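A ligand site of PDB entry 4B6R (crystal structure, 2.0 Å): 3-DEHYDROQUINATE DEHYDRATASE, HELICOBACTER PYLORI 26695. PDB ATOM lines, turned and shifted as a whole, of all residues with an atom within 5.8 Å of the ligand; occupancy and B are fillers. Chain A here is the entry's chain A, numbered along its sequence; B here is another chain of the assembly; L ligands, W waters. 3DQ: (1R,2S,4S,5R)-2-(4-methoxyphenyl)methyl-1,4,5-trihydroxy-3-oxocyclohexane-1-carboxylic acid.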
ATOM      1  N   PRO A   9     -14.762  23.447   0.639  1.00  0.00           N
ATOM      2  CA  PRO A   9     -15.780  23.013   1.591  1.00  0.00           C
ATOM      3  C   PRO A   9     -17.036  22.478   0.908  1.00  0.00           C
ATOM      4  O   PRO A   9     -17.443  22.986  -0.172  1.00  0.00           O
ATOM      5  CB  PRO A   9     -16.063  24.296   2.431  1.00  0.00           C
ATOM      6  CG  PRO A   9     -15.589  25.463   1.518  1.00  0.00           C
ATOM      7  CD  PRO A   9     -14.402  24.878   0.792  1.00  0.00           C
ATOM      8  N   ASN A  10     -17.607  21.422   1.523  1.00  0.00           N
ATOM      9  CA  ASN A  10     -18.864  20.786   1.086  1.00  0.00           C
ATOM     10  C   ASN A  10     -18.778  19.905  -0.147  1.00  0.00           C
ATOM     11  O   ASN A  10     -19.762  19.225  -0.466  1.00  0.00           O
ATOM     12  CB  ASN A  10     -19.976  21.814   0.919  1.00  0.00           C
ATOM     13  CG  ASN A  10     -20.322  22.481   2.201  1.00  0.00           C
ATOM     14  OD1 ASN A  10     -20.489  21.819   3.218  1.00  0.00           O
ATOM     15  ND2 ASN A  10     -20.326  23.812   2.205  1.00  0.00           N
ATOM     16  N   LEU A  11     -17.651  19.939  -0.845  1.00  0.00           N
ATOM     17  CA  LEU A  11     -17.467  19.125  -2.033  1.00  0.00           C
ATOM     18  C   LEU A  11     -17.434  17.618  -1.719  1.00  0.00           C
ATOM     19  O   LEU A  11     -17.897  16.817  -2.535  1.00  0.00           O
ATOM     20  CB  LEU A  11     -16.253  19.580  -2.847  1.00  0.00           C
ATOM     21  CG  LEU A  11     -16.626  20.834  -3.636  1.00  0.00           C
ATOM     22  CD1 LEU A  11     -15.443  21.625  -4.021  1.00  0.00           C
ATOM     23  CD2 LEU A  11     -17.385  20.428  -4.911  1.00  0.00           C
ATOM     24  N   MET A  13     -19.435  16.289  -0.059  1.00  0.00           N
ATOM     25  CA  MET A  13     -20.827  15.909   0.149  1.00  0.00           C
ATOM     26  C   MET A  13     -21.560  15.685  -1.147  1.00  0.00           C
ATOM     27  O   MET A  13     -22.760  15.487  -1.116  1.00  0.00           O
ATOM     28  CB  MET A  13     -21.572  16.982   0.962  1.00  0.00           C
ATOM     29  CG  MET A  13     -21.043  17.164   2.370  1.00  0.00           C
ATOM     30  SD  MET A  13     -20.858  15.679   3.426  1.00  0.00           S
ATOM     31  CE  MET A  13     -22.554  15.284   3.820  1.00  0.00           C
ATOM     32  N   LEU A  14     -20.851  15.746  -2.266  1.00  0.00           N
ATOM     33  CA  LEU A  14     -21.413  15.446  -3.577  1.00  0.00           C
ATOM     34  C   LEU A  14     -22.023  14.046  -3.628  1.00  0.00           C
ATOM     35  O   LEU A  14     -21.488  13.110  -3.023  1.00  0.00           O
ATOM     36  CB  LEU A  14     -20.331  15.522  -4.627  1.00  0.00           C
ATOM     37  CG  LEU A  14     -19.991  16.915  -5.106  1.00  0.00           C
ATOM     38  CD1 LEU A  14     -18.670  16.841  -5.831  1.00  0.00           C
ATOM     39  CD2 LEU A  14     -21.112  17.408  -6.036  1.00  0.00           C
ATOM     40  N   GLY A  15     -23.126  13.924  -4.364  1.00  0.00           N
ATOM     41  CA  GLY A  15     -23.899  12.687  -4.439  1.00  0.00           C
ATOM     42  C   GLY A  15     -24.676  12.381  -3.176  1.00  0.00           C
ATOM     43  O   GLY A  15     -25.558  11.521  -3.179  1.00  0.00           O
ATOM     44  N   ARG A  17     -26.480  14.702  -1.585  1.00  0.00           N
ATOM     45  CA  ARG A  17     -27.468  15.817  -1.548  1.00  0.00           C
ATOM     46  C   ARG A  17     -27.541  16.600  -2.884  1.00  0.00           C
ATOM     47  O   ARG A  17     -26.537  16.702  -3.602  1.00  0.00           O
ATOM     48  CB  ARG A  17     -27.164  16.842  -0.444  1.00  0.00           C
ATOM     49  CG  ARG A  17     -27.354  16.375   1.019  1.00  0.00           C
ATOM     50  CD  ARG A  17     -28.798  16.086   1.442  1.00  0.00           C
ATOM     51  NE  ARG A  17     -28.825  15.433   2.752  1.00  0.00           N
ATOM     52  CZ  ARG A  17     -29.903  14.852   3.303  1.00  0.00           C
ATOM     53  NH1 ARG A  17     -31.066  14.859   2.664  1.00  0.00           N
ATOM     54  NH2 ARG A  17     -29.808  14.280   4.496  1.00  0.00           N
ATOM     55  N   ASP A  18     -28.736  17.125  -3.201  1.00  0.00           N
ATOM     56  CA  ASP A  18     -28.980  18.255  -4.171  1.00  0.00           C
ATOM     57  C   ASP A  18     -28.793  18.104  -5.714  1.00  0.00           C
ATOM     58  O   ASP A  18     -28.281  19.051  -6.355  1.00  0.00           O
ATOM     59  CB  ASP A  18     -28.230  19.547  -3.705  1.00  0.00           C
ATOM     60  CG  ASP A  18     -28.612  19.983  -2.276  1.00  0.00           C
ATOM     61  OD1 ASP A  18     -29.573  19.418  -1.684  1.00  0.00           O
ATOM     62  OD2 ASP A  18     -27.938  20.905  -1.733  1.00  0.00           O
ATOM     63  N   TYR A  22     -25.987  19.772  -9.226  1.00  0.00           N
ATOM     64  CA  TYR A  22     -24.891  18.901  -8.781  1.00  0.00           C
ATOM     65  C   TYR A  22     -24.939  17.441  -9.253  1.00  0.00           C
ATOM     66  O   TYR A  22     -23.929  16.753  -9.183  1.00  0.00           O
ATOM     67  CB  TYR A  22     -24.755  18.962  -7.241  1.00  0.00           C
ATOM     68  CG  TYR A  22     -24.624  20.364  -6.709  1.00  0.00           C
ATOM     69  CD1 TYR A  22     -23.470  21.118  -6.940  1.00  0.00           C
ATOM     70  CD2 TYR A  22     -25.686  20.981  -6.008  1.00  0.00           C
ATOM     71  CE1 TYR A  22     -23.357  22.429  -6.479  1.00  0.00           C
ATOM     72  CE2 TYR A  22     -25.572  22.309  -5.533  1.00  0.00           C
ATOM     73  CZ  TYR A  22     -24.395  23.031  -5.777  1.00  0.00           C
ATOM     74  OH  TYR A  22     -24.266  24.343  -5.305  1.00  0.00           O
ATOM     75  N   ASN A  76     -10.838  23.689  -6.657  1.00  0.00           N
ATOM     76  CA  ASN A  76     -12.199  24.175  -6.507  1.00  0.00           C
ATOM     77  C   ASN A  76     -12.391  24.697  -5.062  1.00  0.00           C
ATOM     78  O   ASN A  76     -12.657  23.906  -4.156  1.00  0.00           O
ATOM     79  CB  ASN A  76     -13.211  23.068  -6.851  1.00  0.00           C
ATOM     80  CG  ASN A  76     -14.684  23.539  -6.782  1.00  0.00           C
ATOM     81  OD1 ASN A  76     -15.028  24.624  -6.229  1.00  0.00           O
ATOM     82  ND2 ASN A  76     -15.573  22.723  -7.356  1.00  0.00           N
ATOM     83  N   PRO A  77     -12.216  26.021  -4.840  1.00  0.00           N
ATOM     84  CA  PRO A  77     -12.279  26.538  -3.462  1.00  0.00           C
ATOM     85  C   PRO A  77     -13.663  26.571  -2.910  1.00  0.00           C
ATOM     86  O   PRO A  77     -13.880  26.952  -1.739  1.00  0.00           O
ATOM     87  CB  PRO A  77     -11.696  27.941  -3.569  1.00  0.00           C
ATOM     88  CG  PRO A  77     -11.038  27.975  -4.899  1.00  0.00           C
ATOM     89  CD  PRO A  77     -11.897  27.114  -5.765  1.00  0.00           C
ATOM     90  N   GLY A  78     -14.624  26.138  -3.700  1.00  0.00           N
ATOM     91  CA  GLY A  78     -16.025  26.094  -3.222  1.00  0.00           C
ATOM     92  C   GLY A  78     -16.504  27.514  -2.806  1.00  0.00           C
ATOM     93  O   GLY A  78     -16.201  28.470  -3.495  1.00  0.00           O
ATOM     94  N   ALA A  79     -17.231  27.646  -1.696  1.00  0.00           N
ATOM     95  CA  ALA A  79     -17.766  28.935  -1.308  1.00  0.00           C
ATOM     96  C   ALA A  79     -16.662  29.929  -0.929  1.00  0.00           C
ATOM     97  O   ALA A  79     -16.904  31.173  -0.957  1.00  0.00           O
ATOM     98  CB  ALA A  79     -18.797  28.800  -0.132  1.00  0.00           C
ATOM     99  N   PHE A  80     -15.482  29.423  -0.590  1.00  0.00           N
ATOM    100  CA  PHE A  80     -14.349  30.298  -0.262  1.00  0.00           C
ATOM    101  C   PHE A  80     -13.867  31.084  -1.455  1.00  0.00           C
ATOM    102  O   PHE A  80     -13.139  32.070  -1.270  1.00  0.00           O
ATOM    103  CB  PHE A  80     -13.151  29.523   0.310  1.00  0.00           C
ATOM    104  CG  PHE A  80     -13.427  28.796   1.621  1.00  0.00           C
ATOM    105  CD1 PHE A  80     -14.375  29.277   2.524  1.00  0.00           C
ATOM    106  CD2 PHE A  80     -12.700  27.653   1.959  1.00  0.00           C
ATOM    107  CE1 PHE A  80     -14.626  28.593   3.757  1.00  0.00           C
ATOM    108  CE2 PHE A  80     -12.963  26.963   3.194  1.00  0.00           C
ATOM    109  CZ  PHE A  80     -13.921  27.423   4.059  1.00  0.00           C
ATOM    110  N   SER A  81     -14.222  30.647  -2.665  1.00  0.00           N
ATOM    111  CA  SER A  81     -13.903  31.388  -3.881  1.00  0.00           C
ATOM    112  C   SER A  81     -14.340  32.836  -3.745  1.00  0.00           C
ATOM    113  O   SER A  81     -13.640  33.731  -4.212  1.00  0.00           O
ATOM    114  CB  SER A  81     -14.659  30.807  -5.126  1.00  0.00           C
ATOM    115  OG  SER A  81     -14.252  29.453  -5.388  1.00  0.00           O
ATOM    116  N   HIS A  82     -15.538  33.038  -3.198  1.00  0.00           N
ATOM    117  CA  HIS A  82     -16.190  34.349  -3.250  1.00  0.00           C
ATOM    118  C   HIS A  82     -15.737  35.253  -2.141  1.00  0.00           C
ATOM    119  O   HIS A  82     -16.015  36.442  -2.165  1.00  0.00           O
ATOM    120  CB  HIS A  82     -17.708  34.175  -3.180  1.00  0.00           C
ATOM    121  CG  HIS A  82     -18.193  33.036  -4.001  1.00  0.00           C
ATOM    122  ND1 HIS A  82     -18.002  32.982  -5.363  1.00  0.00           N
ATOM    123  CD2 HIS A  82     -18.808  31.865  -3.653  1.00  0.00           C
ATOM    124  CE1 HIS A  82     -18.486  31.841  -5.826  1.00  0.00           C
ATOM    125  NE2 HIS A  82     -19.002  31.162  -4.810  1.00  0.00           N
ATOM    126  N   VAL A 101     -11.617  25.460 -10.942  1.00  0.00           N
ATOM    127  CA  VAL A 101     -12.741  24.761 -11.536  1.00  0.00           C
ATOM    128  C   VAL A 101     -13.996  24.943 -10.667  1.00  0.00           C
ATOM    129  O   VAL A 101     -13.925  24.823  -9.446  1.00  0.00           O
ATOM    130  CB  VAL A 101     -12.488  23.220 -11.603  1.00  0.00           C
ATOM    131  CG1 VAL A 101     -13.756  22.477 -12.121  1.00  0.00           C
ATOM    132  CG2 VAL A 101     -11.242  22.876 -12.496  1.00  0.00           C
ATOM    133  N   HIS A 102     -15.132  25.232 -11.285  1.00  0.00           N
ATOM    134  CA  HIS A 102     -16.377  25.119 -10.582  1.00  0.00           C
ATOM    135  C   HIS A 102     -17.262  24.133 -11.308  1.00  0.00           C
ATOM    136  O   HIS A 102     -17.346  24.169 -12.520  1.00  0.00           O
ATOM    137  CB  HIS A 102     -17.107  26.461 -10.485  1.00  0.00           C
ATOM    138  CG  HIS A 102     -16.293  27.523  -9.841  1.00  0.00           C
ATOM    139  ND1 HIS A 102     -16.206  27.657  -8.472  1.00  0.00           N
ATOM    140  CD2 HIS A 102     -15.458  28.450 -10.370  1.00  0.00           C
ATOM    141  CE1 HIS A 102     -15.362  28.640  -8.190  1.00  0.00           C
ATOM    142  NE2 HIS A 102     -14.888  29.121  -9.323  1.00  0.00           N
ATOM    143  N   LEU A 103     -17.958  23.296 -10.546  1.00  0.00           N
ATOM    144  CA  LEU A 103     -18.970  22.414 -11.164  1.00  0.00           C
ATOM    145  C   LEU A 103     -20.068  23.239 -11.835  1.00  0.00           C
ATOM    146  O   LEU A 103     -20.518  22.905 -12.932  1.00  0.00           O
ATOM    147  CB  LEU A 103     -19.646  21.546 -10.087  1.00  0.00           C
ATOM    148  CG  LEU A 103     -18.757  20.487  -9.422  1.00  0.00           C
ATOM    149  CD1 LEU A 103     -19.516  19.870  -8.246  1.00  0.00           C
ATOM    150  CD2 LEU A 103     -18.385  19.407 -10.470  1.00  0.00           C
ATOM    151  N   THR A 104     -20.531  24.288 -11.155  1.00  0.00           N
ATOM    152  CA  THR A 104     -21.678  25.047 -11.638  1.00  0.00           C
ATOM    153  C   THR A 104     -21.225  26.345 -12.297  1.00  0.00           C
ATOM    154  O   THR A 104     -20.076  26.736 -12.143  1.00  0.00           O
ATOM    155  CB  THR A 104     -22.703  25.389 -10.481  1.00  0.00           C
ATOM    156  OG1 THR A 104     -22.091  26.270  -9.536  1.00  0.00           O
ATOM    157  CG2 THR A 104     -23.144  24.081  -9.749  1.00  0.00           C
ATOM    158  N   ASN A 105     -22.113  26.990 -13.031  1.00  0.00           N
ATOM    159  CA  ASN A 105     -21.781  28.245 -13.685  1.00  0.00           C
ATOM    160  C   ASN A 105     -22.034  29.359 -12.694  1.00  0.00           C
ATOM    161  O   ASN A 105     -23.200  29.696 -12.388  1.00  0.00           O
ATOM    162  CB  ASN A 105     -22.630  28.423 -14.937  1.00  0.00           C
ATOM    163  CG  ASN A 105     -22.273  29.642 -15.750  1.00  0.00           C
ATOM    164  OD1 ASN A 105     -21.561  30.560 -15.301  1.00  0.00           O
ATOM    165  ND2 ASN A 105     -22.803  29.680 -16.962  1.00  0.00           N
ATOM    166  N   ILE A 106     -20.964  29.904 -12.131  1.00  0.00           N
ATOM    167  CA  ILE A 106     -21.156  30.922 -11.095  1.00  0.00           C
ATOM    168  C   ILE A 106     -21.561  32.311 -11.578  1.00  0.00           C
ATOM    169  O   ILE A 106     -21.827  33.176 -10.742  1.00  0.00           O
ATOM    170  CB  ILE A 106     -19.963  31.046 -10.116  1.00  0.00           C
ATOM    171  CG1 ILE A 106     -18.655  31.329 -10.856  1.00  0.00           C
ATOM    172  CG2 ILE A 106     -19.929  29.786  -9.253  1.00  0.00           C
ATOM    173  CD1 ILE A 106     -17.490  31.880  -9.986  1.00  0.00           C
ATOM    174  N   ARG A 109     -25.887  32.250 -11.049  1.00  0.00           N
ATOM    175  CA  ARG A 109     -26.526  31.840  -9.800  1.00  0.00           C
ATOM    176  C   ARG A 109     -26.774  33.101  -8.957  1.00  0.00           C
ATOM    177  O   ARG A 109     -26.992  34.138  -9.542  1.00  0.00           O
ATOM    178  CB  ARG A 109     -25.662  30.775  -9.099  1.00  0.00           C
ATOM    179  CG  ARG A 109     -25.407  29.501  -9.934  1.00  0.00           C
ATOM    180  CD  ARG A 109     -24.681  28.407  -9.112  1.00  0.00           C
ATOM    181  NE  ARG A 109     -25.416  28.056  -7.889  1.00  0.00           N
ATOM    182  CZ  ARG A 109     -24.947  27.233  -6.943  1.00  0.00           C
ATOM    183  NH1 ARG A 109     -23.745  26.663  -7.046  1.00  0.00           N
ATOM    184  NH2 ARG A 109     -25.695  26.985  -5.872  1.00  0.00           N
ATOM    185  N   ARG A 113     -22.381  34.809  -5.477  1.00  0.00           N
ATOM    186  CA  ARG A 113     -21.434  33.853  -6.098  1.00  0.00           C
ATOM    187  C   ARG A 113     -20.663  34.406  -7.305  1.00  0.00           C
ATOM    188  O   ARG A 113     -19.785  33.722  -7.830  1.00  0.00           O
ATOM    189  CB  ARG A 113     -22.127  32.525  -6.500  1.00  0.00           C
ATOM    190  CG  ARG A 113     -22.763  31.774  -5.315  1.00  0.00           C
ATOM    191  CD  ARG A 113     -23.192  30.334  -5.705  1.00  0.00           C
ATOM    192  NE  ARG A 113     -24.186  29.832  -4.765  1.00  0.00           N
ATOM    193  CZ  ARG A 113     -23.900  29.184  -3.616  1.00  0.00           C
ATOM    194  NH1 ARG A 113     -22.661  28.873  -3.296  1.00  0.00           N
ATOM    195  NH2 ARG A 113     -24.884  28.822  -2.813  1.00  0.00           N
ATOM    196  N   TYR A 134     -13.130  19.052 -14.456  1.00  0.00           N
ATOM    197  CA  TYR A 134     -11.852  18.626 -13.876  1.00  0.00           C
ATOM    198  C   TYR A 134     -10.917  17.949 -14.920  1.00  0.00           C
ATOM    199  O   TYR A 134      -9.693  18.105 -14.856  1.00  0.00           O
ATOM    200  CB  TYR A 134     -12.088  17.699 -12.677  1.00  0.00           C
ATOM    201  CG  TYR A 134     -12.671  18.384 -11.439  1.00  0.00           C
ATOM    202  CD1 TYR A 134     -11.856  19.099 -10.564  1.00  0.00           C
ATOM    203  CD2 TYR A 134     -14.038  18.362 -11.194  1.00  0.00           C
ATOM    204  CE1 TYR A 134     -12.396  19.733  -9.441  1.00  0.00           C
ATOM    205  CE2 TYR A 134     -14.589  19.005 -10.072  1.00  0.00           C
ATOM    206  CZ  TYR A 134     -13.761  19.675  -9.196  1.00  0.00           C
ATOM    207  OH  TYR A 134     -14.322  20.275  -8.072  1.00  0.00           O
ATOM    208  N   ILE B  85     -20.603  31.951   3.490  1.00  0.00           N
ATOM    209  CA  ILE B  85     -21.393  31.278   2.449  1.00  0.00           C
ATOM    210  C   ILE B  85     -21.206  29.743   2.605  1.00  0.00           C
ATOM    211  O   ILE B  85     -22.101  28.965   2.289  1.00  0.00           O
ATOM    212  CB  ILE B  85     -20.994  31.761   1.012  1.00  0.00           C
ATOM    213  CG1 ILE B  85     -21.193  33.298   0.909  1.00  0.00           C
ATOM    214  CG2 ILE B  85     -21.820  31.041  -0.060  1.00  0.00           C
ATOM    215  CD1 ILE B  85     -20.601  33.888  -0.393  1.00  0.00           C
ATOM    216  N   ASP B  89     -24.055  26.937   2.886  1.00  0.00           N
ATOM    217  CA  ASP B  89     -24.198  25.817   1.947  1.00  0.00           C
ATOM    218  C   ASP B  89     -24.334  24.455   2.750  1.00  0.00           C
ATOM    219  O   ASP B  89     -25.128  23.580   2.401  1.00  0.00           O
ATOM    220  CB  ASP B  89     -23.013  25.746   0.955  1.00  0.00           C
ATOM    221  CG  ASP B  89     -23.124  26.751  -0.237  1.00  0.00           C
ATOM    222  OD1 ASP B  89     -24.210  27.313  -0.558  1.00  0.00           O
ATOM    223  OD2 ASP B  89     -22.068  26.968  -0.900  1.00  0.00           O
ATOM    224  N   LEU B  93     -27.495  21.576   2.764  1.00  0.00           N
ATOM    225  CA  LEU B  93     -27.440  20.127   2.551  1.00  0.00           C
ATOM    226  C   LEU B  93     -27.717  19.244   3.790  1.00  0.00           C
ATOM    227  O   LEU B  93     -27.635  18.012   3.715  1.00  0.00           O
ATOM    228  CB  LEU B  93     -26.136  19.727   1.848  1.00  0.00           C
ATOM    229  CG  LEU B  93     -24.771  20.057   2.458  1.00  0.00           C
ATOM    230  CD1 LEU B  93     -24.378  19.118   3.619  1.00  0.00           C
ATOM    231  CD2 LEU B  93     -23.693  20.054   1.369  1.00  0.00           C
HETATM  232  CAA 3DQ L   1     -23.498  18.915  -2.289  1.00  0.00           C
HETATM  233  OAN 3DQ L   1     -22.702  19.994  -1.800  1.00  0.00           O
HETATM  234  CAR 3DQ L   1     -22.289  20.996  -2.642  1.00  0.00           C
HETATM  235  CAK 3DQ L   1     -22.611  22.335  -2.397  1.00  0.00           C
HETATM  236  CAI 3DQ L   1     -22.150  23.327  -3.290  1.00  0.00           C
HETATM  237  CAJ 3DQ L   1     -21.504  20.654  -3.746  1.00  0.00           C
HETATM  238  CAH 3DQ L   1     -21.067  21.649  -4.622  1.00  0.00           C
HETATM  239  CAQ 3DQ L   1     -21.361  23.001  -4.421  1.00  0.00           C
HETATM  240  CAL 3DQ L   1     -20.890  24.055  -5.443  1.00  0.00           C
HETATM  241  CAU 3DQ L   1     -19.499  24.672  -5.241  1.00  0.00           C
HETATM  242  CAP 3DQ L   1     -19.702  25.427  -3.983  1.00  0.00           C
HETATM  243  OAC 3DQ L   1     -19.379  24.889  -2.937  1.00  0.00           O
HETATM  244  CAT 3DQ L   1     -20.347  26.801  -4.052  1.00  0.00           C
HETATM  245  OAF 3DQ L   1     -20.317  27.461  -2.773  1.00  0.00           O
HETATM  246  CAS 3DQ L   1     -19.733  27.660  -5.161  1.00  0.00           C
HETATM  247  OAE 3DQ L   1     -20.524  28.833  -5.227  1.00  0.00           O
HETATM  248  CAM 3DQ L   1     -19.763  26.931  -6.540  1.00  0.00           C
HETATM  249  CAV 3DQ L   1     -19.006  25.585  -6.409  1.00  0.00           C
HETATM  250  CAO 3DQ L   1     -19.022  24.786  -7.694  1.00  0.00           C
HETATM  251  OAB 3DQ L   1     -19.810  25.089  -8.617  1.00  0.00           O
HETATM  252  OAD 3DQ L   1     -18.208  23.855  -7.759  1.00  0.00           O
HETATM  253  OAG 3DQ L   1     -17.633  25.955  -6.263  1.00  0.00           O
HETATM  254  O   HOH W   1     -25.262  22.909  -0.199  1.00  0.00           O
HETATM  255  O   HOH W   2     -19.117  25.217  -0.081  1.00  0.00           O
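A ring nitrogen (ND1) of His 102 lies within hydrogen-bond range of an oxygen (OAG) of the ligand (3.1 Å).
ND2 of Asn 76 is in hydrogen-bond range of OAD of the ligand.
N of Leu 103 lies within hydrogen-bond range of OAD of the ligand (2.9 Å).
An oxygen (OAF) of the ligand sits at hydrogen-bond distance from the backbone NH of Ala 79, at 3.3 Å.
The backbone NH of Thr 104 sits at hydrogen-bond distance from an oxygen (OAB) of the ligand, at 2.8 Å.
A ring nitrogen (NE2) of His 82 lies within hydrogen-bond range of an oxygen (OAE) of the ligand (2.8 Å).
The side-chain carboxylate (OD2) of Asp 89 of chain B lies within hydrogen-bond range of an oxygen (OAF) of the ligand (2.6 Å).
The guanidinium group (NH1) of Arg 113 sits at hydrogen-bond distance from an oxygen (OAF) of the ligand, at 2.8 Å.
An oxygen (OAB) of the ligand sits at hydrogen-bond distance from the side-chain hydroxyl of Thr 104, 2.7 Å away.
The guanidinium group (NE) of Arg 17 lies within hydrogen-bond range of the backbone carbonyl oxygen (O) of Leu 93 of chain B.
O of Val 101 lies close to ND2 of Asn 76, at 3.4 Å.
The backbone carbonyl oxygen of Gly 78 sits at hydrogen-bond distance from the side-chain hydroxyl of Ser 81 (2.9 Å).
OH of Tyr 22 sits at hydrogen-bond distance from NH1 of Arg 109 (2.9 Å).
The side-chain carboxylate of Asp 89 of chain B lies within salt-bridge range of the guanidinium group of Arg 113.
The backbone carbonyl oxygen (O) of Arg 113 lies close to a ring nitrogen (ND1) of His 82 (3.1 Å).
The guanidinium group of Arg 109 lies within hydrogen-bond range of the side-chain hydroxyl of Thr 104 (3.0 Å).
The side-chain amide oxygen (OD1) of Asn 76 lies within hydrogen-bond range of the backbone NH (N) of Gly 78 (3.0 Å).
An oxygen (OAN) of the ligand lies close to the backbone carbonyl oxygen (O) of Asn 10, at 3.3 Å.
Pro 9 touches the ligand (O to OAC, 3.9 Å).
Leu 11 touches the ligand.
Met 13 touches the ligand.
Leu 14 touches the ligand (CD2 to CAJ, 3.99 Å).
O of Arg 17 touches CAA of the ligand (3.98 Å).
Tyr 22 touches the ligand.
CA of Gly 78 touches OAG of the ligand, at 3.4 Å.
Ile 106 touches the ligand (CG2 to CAM, 3.9 Å).
Leu 93 of chain B touches the ligand.
Hydrophobic or aromatic side chains within 4 Å of the ligand: Leu 11, Leu 14, Tyr 22, Ala 79, His 82, His 102, Leu 103, Ile 106 and Leu 93 of chain B.
18 residues have an atom within 4 Å of the ligand: Pro 9, Asn 10, Leu 11, Met 13, Leu 14, Arg 17, Tyr 22, Asn 76, Gly 78, Ala 79, His 82, His 102, Leu 103, Thr 104, Ile 106, Arg 113, Asp 89 of chain B and Leu 93 of chain B.
Water W2 lies within hydrogen-bond range of the backbone carbonyl oxygen of Pro 9 (2.8 Å), an oxygen (OAC) of the ligand (2.9 Å), the side-chain amide nitrogen of Asn 10 (2.9 Å) and the backbone NH of Ala 79 (3.5 Å).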
